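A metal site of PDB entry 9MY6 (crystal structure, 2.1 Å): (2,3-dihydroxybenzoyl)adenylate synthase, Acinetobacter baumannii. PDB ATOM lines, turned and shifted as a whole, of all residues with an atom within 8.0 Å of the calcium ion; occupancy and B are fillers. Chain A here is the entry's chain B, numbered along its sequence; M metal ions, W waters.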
ATOM      1  N   VAL A 300     -18.143  19.246 -12.122  1.00  0.00           N
ATOM      2  CA  VAL A 300     -17.084  18.528 -12.803  1.00  0.00           C
ATOM      3  C   VAL A 300     -17.144  18.820 -14.290  1.00  0.00           C
ATOM      4  O   VAL A 300     -18.213  18.760 -14.908  1.00  0.00           O
ATOM      5  CB  VAL A 300     -17.210  17.031 -12.513  1.00  0.00           C
ATOM      6  CG1 VAL A 300     -16.207  16.248 -13.366  1.00  0.00           C
ATOM      7  CG2 VAL A 300     -16.993  16.808 -11.033  1.00  0.00           C
ATOM      8  N   ASN A 301     -16.008  19.117 -14.897  1.00  0.00           N
ATOM      9  CA  ASN A 301     -16.001  19.356 -16.325  1.00  0.00           C
ATOM     10  C   ASN A 301     -15.092  18.397 -17.053  1.00  0.00           C
ATOM     11  O   ASN A 301     -14.992  18.484 -18.280  1.00  0.00           O
ATOM     12  CB  ASN A 301     -15.650  20.833 -16.645  1.00  0.00           C
ATOM     13  CG  ASN A 301     -14.359  21.291 -15.950  1.00  0.00           C
ATOM     14  OD1 ASN A 301     -13.423  20.506 -15.801  1.00  0.00           O
ATOM     15  ND2 ASN A 301     -14.311  22.543 -15.561  1.00  0.00           N
ATOM     16  N   LYS A 321     -29.487  13.896 -18.111  1.00  0.00           N
ATOM     17  CA  LYS A 321     -28.742  14.831 -18.931  1.00  0.00           C
ATOM     18  C   LYS A 321     -28.365  16.059 -18.128  1.00  0.00           C
ATOM     19  O   LYS A 321     -27.234  16.557 -18.236  1.00  0.00           O
ATOM     20  CB  LYS A 321     -29.550  15.214 -20.176  1.00  0.00           C
ATOM     21  CG  LYS A 321     -29.110  14.462 -21.438  1.00  0.00           C
ATOM     22  CD  LYS A 321     -29.798  14.965 -22.700  1.00  0.00           C
ATOM     23  N   ILE A 324     -25.216  15.998 -15.781  1.00  0.00           N
ATOM     24  CA  ILE A 324     -23.901  15.841 -16.362  1.00  0.00           C
ATOM     25  C   ILE A 324     -23.643  16.854 -17.473  1.00  0.00           C
ATOM     26  O   ILE A 324     -22.659  16.707 -18.214  1.00  0.00           O
ATOM     27  CB  ILE A 324     -23.694  14.408 -16.852  1.00  0.00           C
ATOM     28  CG1 ILE A 324     -24.712  14.085 -17.940  1.00  0.00           C
ATOM     29  CG2 ILE A 324     -23.857  13.436 -15.704  1.00  0.00           C
ATOM     30  CD1 ILE A 324     -24.207  13.032 -18.895  1.00  0.00           C
ATOM     31  N   GLN A 325     -24.493  17.871 -17.616  1.00  0.00           N
ATOM     32  CA  GLN A 325     -24.256  18.874 -18.654  1.00  0.00           C
ATOM     33  C   GLN A 325     -22.848  19.483 -18.571  1.00  0.00           C
ATOM     34  O   GLN A 325     -22.217  19.742 -19.607  1.00  0.00           O
ATOM     35  CB  GLN A 325     -25.285  19.991 -18.556  1.00  0.00           C
ATOM     36  CG  GLN A 325     -26.740  19.677 -19.050  1.00  0.00           C
ATOM     37  CD  GLN A 325     -26.929  19.155 -20.506  1.00  0.00           C
ATOM     38  OE1 GLN A 325     -25.996  18.647 -21.155  1.00  0.00           O
ATOM     39  NE2 GLN A 325     -28.168  19.282 -21.005  1.00  0.00           N
ATOM     40  N   SER A 326     -22.324  19.701 -17.349  1.00  0.00           N
ATOM     41  CA  SER A 326     -21.066  20.449 -17.194  1.00  0.00           C
ATOM     42  C   SER A 326     -19.856  19.656 -17.653  1.00  0.00           C
ATOM     43  O   SER A 326     -18.771  20.247 -17.775  1.00  0.00           O
ATOM     44  CB  SER A 326     -20.847  20.875 -15.744  1.00  0.00           C
ATOM     45  OG  SER A 326     -20.514  19.767 -14.931  1.00  0.00           O
ATOM     46  N   LEU A 327     -19.983  18.347 -17.872  1.00  0.00           N
ATOM     47  CA  LEU A 327     -18.847  17.609 -18.405  1.00  0.00           C
ATOM     48  C   LEU A 327     -18.434  18.215 -19.723  1.00  0.00           C
ATOM     49  O   LEU A 327     -19.258  18.362 -20.604  1.00  0.00           O
ATOM     50  CB  LEU A 327     -19.188  16.154 -18.637  1.00  0.00           C
ATOM     51  CG  LEU A 327     -19.109  15.205 -17.464  1.00  0.00           C
ATOM     52  CD1 LEU A 327     -19.594  13.806 -17.910  1.00  0.00           C
ATOM     53  CD2 LEU A 327     -17.718  15.160 -17.013  1.00  0.00           C
ATOM     54  N   LYS A 328     -17.156  18.556 -19.866  1.00  0.00           N
ATOM     55  CA  LYS A 328     -16.702  19.096 -21.134  1.00  0.00           C
ATOM     56  C   LYS A 328     -15.845  18.115 -21.918  1.00  0.00           C
ATOM     57  O   LYS A 328     -15.816  18.177 -23.139  1.00  0.00           O
ATOM     58  CB  LYS A 328     -15.912  20.409 -20.902  1.00  0.00           C
ATOM     59  CG  LYS A 328     -16.792  21.487 -20.270  1.00  0.00           C
ATOM     60  CD  LYS A 328     -16.393  22.883 -20.730  1.00  0.00           C
ATOM     61  CE  LYS A 328     -15.224  23.399 -19.985  1.00  0.00           C
ATOM     62  NZ  LYS A 328     -15.344  24.887 -19.753  1.00  0.00           N
ATOM     63  N   LEU A 329     -15.200  17.189 -21.247  1.00  0.00           N
ATOM     64  CA  LEU A 329     -14.221  16.343 -21.912  1.00  0.00           C
ATOM     65  C   LEU A 329     -14.197  15.038 -21.170  1.00  0.00           C
ATOM     66  O   LEU A 329     -14.156  15.040 -19.942  1.00  0.00           O
ATOM     67  CB  LEU A 329     -12.813  16.998 -21.933  1.00  0.00           C
ATOM     68  CG  LEU A 329     -11.615  16.170 -22.435  1.00  0.00           C
ATOM     69  CD1 LEU A 329     -11.752  15.890 -23.939  1.00  0.00           C
ATOM     70  CD2 LEU A 329     -10.296  16.885 -22.171  1.00  0.00           C
ATOM     71  N   PRO A 346     -20.218  12.121 -27.523  1.00  0.00           N
ATOM     72  CA  PRO A 346     -20.794  13.464 -27.691  1.00  0.00           C
ATOM     73  C   PRO A 346     -22.316  13.481 -27.810  1.00  0.00           C
ATOM     74  O   PRO A 346     -22.956  14.440 -27.360  1.00  0.00           O
ATOM     75  CB  PRO A 346     -20.124  13.972 -28.980  1.00  0.00           C
ATOM     76  CG  PRO A 346     -19.618  12.723 -29.676  1.00  0.00           C
ATOM     77  CD  PRO A 346     -19.289  11.754 -28.602  1.00  0.00           C
ATOM     78  N   LEU A 349     -23.488  11.762 -23.792  1.00  0.00           N
ATOM     79  CA  LEU A 349     -22.863  12.416 -22.645  1.00  0.00           C
ATOM     80  C   LEU A 349     -22.668  13.906 -22.853  1.00  0.00           C
ATOM     81  O   LEU A 349     -22.332  14.612 -21.911  1.00  0.00           O
ATOM     82  CB  LEU A 349     -21.513  11.764 -22.321  1.00  0.00           C
ATOM     83  CG  LEU A 349     -21.662  10.272 -21.974  1.00  0.00           C
ATOM     84  CD1 LEU A 349     -20.328   9.587 -21.685  1.00  0.00           C
ATOM     85  CD2 LEU A 349     -22.652  10.077 -20.802  1.00  0.00           C
ATOM     86  N   ASN A 350     -22.872  14.392 -24.072  1.00  0.00           N
ATOM     87  CA  ASN A 350     -22.847  15.825 -24.316  1.00  0.00           C
ATOM     88  C   ASN A 350     -21.497  16.401 -23.897  1.00  0.00           C
ATOM     89  O   ASN A 350     -21.417  17.383 -23.157  1.00  0.00           O
ATOM     90  CB  ASN A 350     -24.034  16.495 -23.607  1.00  0.00           C
ATOM     91  CG  ASN A 350     -25.393  15.868 -24.029  1.00  0.00           C
ATOM     92  OD1 ASN A 350     -25.463  15.250 -25.077  1.00  0.00           O
ATOM     93  ND2 ASN A 350     -26.431  15.995 -23.207  1.00  0.00           N
ATOM     94  N   CYS A 351     -20.434  15.779 -24.371  1.00  0.00           N
ATOM     95  CA  CYS A 351     -19.088  16.278 -24.118  1.00  0.00           C
ATOM     96  C   CYS A 351     -18.170  15.756 -25.198  1.00  0.00           C
ATOM     97  O   CYS A 351     -18.517  14.846 -25.966  1.00  0.00           O
ATOM     98  CB  CYS A 351     -18.576  15.866 -22.739  1.00  0.00           C
ATOM     99  SG  CYS A 351     -18.418  14.065 -22.640  1.00  0.00           S
ATOM    100  N   LYS A 352     -16.974  16.339 -25.250  1.00  0.00           N
ATOM    101  CA  LYS A 352     -15.960  15.984 -26.220  1.00  0.00           C
ATOM    102  C   LYS A 352     -15.328  14.663 -25.845  1.00  0.00           C
ATOM    103  O   LYS A 352     -15.214  14.324 -24.663  1.00  0.00           O
ATOM    104  CB  LYS A 352     -14.894  17.071 -26.308  1.00  0.00           C
ATOM    105  CG  LYS A 352     -13.812  16.777 -27.329  1.00  0.00           C
ATOM    106  CD  LYS A 352     -13.588  17.977 -28.230  1.00  0.00           C
ATOM    107  CE  LYS A 352     -12.354  17.793 -29.110  1.00  0.00           C
ATOM    108  NZ  LYS A 352     -12.750  17.558 -30.527  1.00  0.00           N
HETATM  109 CA    CA M   1     -21.323  18.990 -21.559  1.00  0.00          CA
HETATM  110  O   HOH W   1     -22.218  17.048 -20.656  1.00  0.00           O
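OD1 of Asn 350 lies close to O of Pro 346 (3.5 Å).
N of Leu 327 lies within hydrogen-bond range of O of Val 300, at 3.5 Å.
Within 4 Å of the calcium ion: Gln 325, Leu 327 and Asn 350.
The nearest printed residue that does not touch the calcium ion is Ser 326 (4.2 Å).
The calcium ion is bound by O of Asn 350 (2.3 Å), O of Gln 325 (2.3 Å), water W1 (2.3 Å) and O of Leu 327 (2.4 Å).
Water W1 bridges the backbone carbonyl oxygen of Ile 324 and the backbone carbonyl oxygen of Leu 349.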
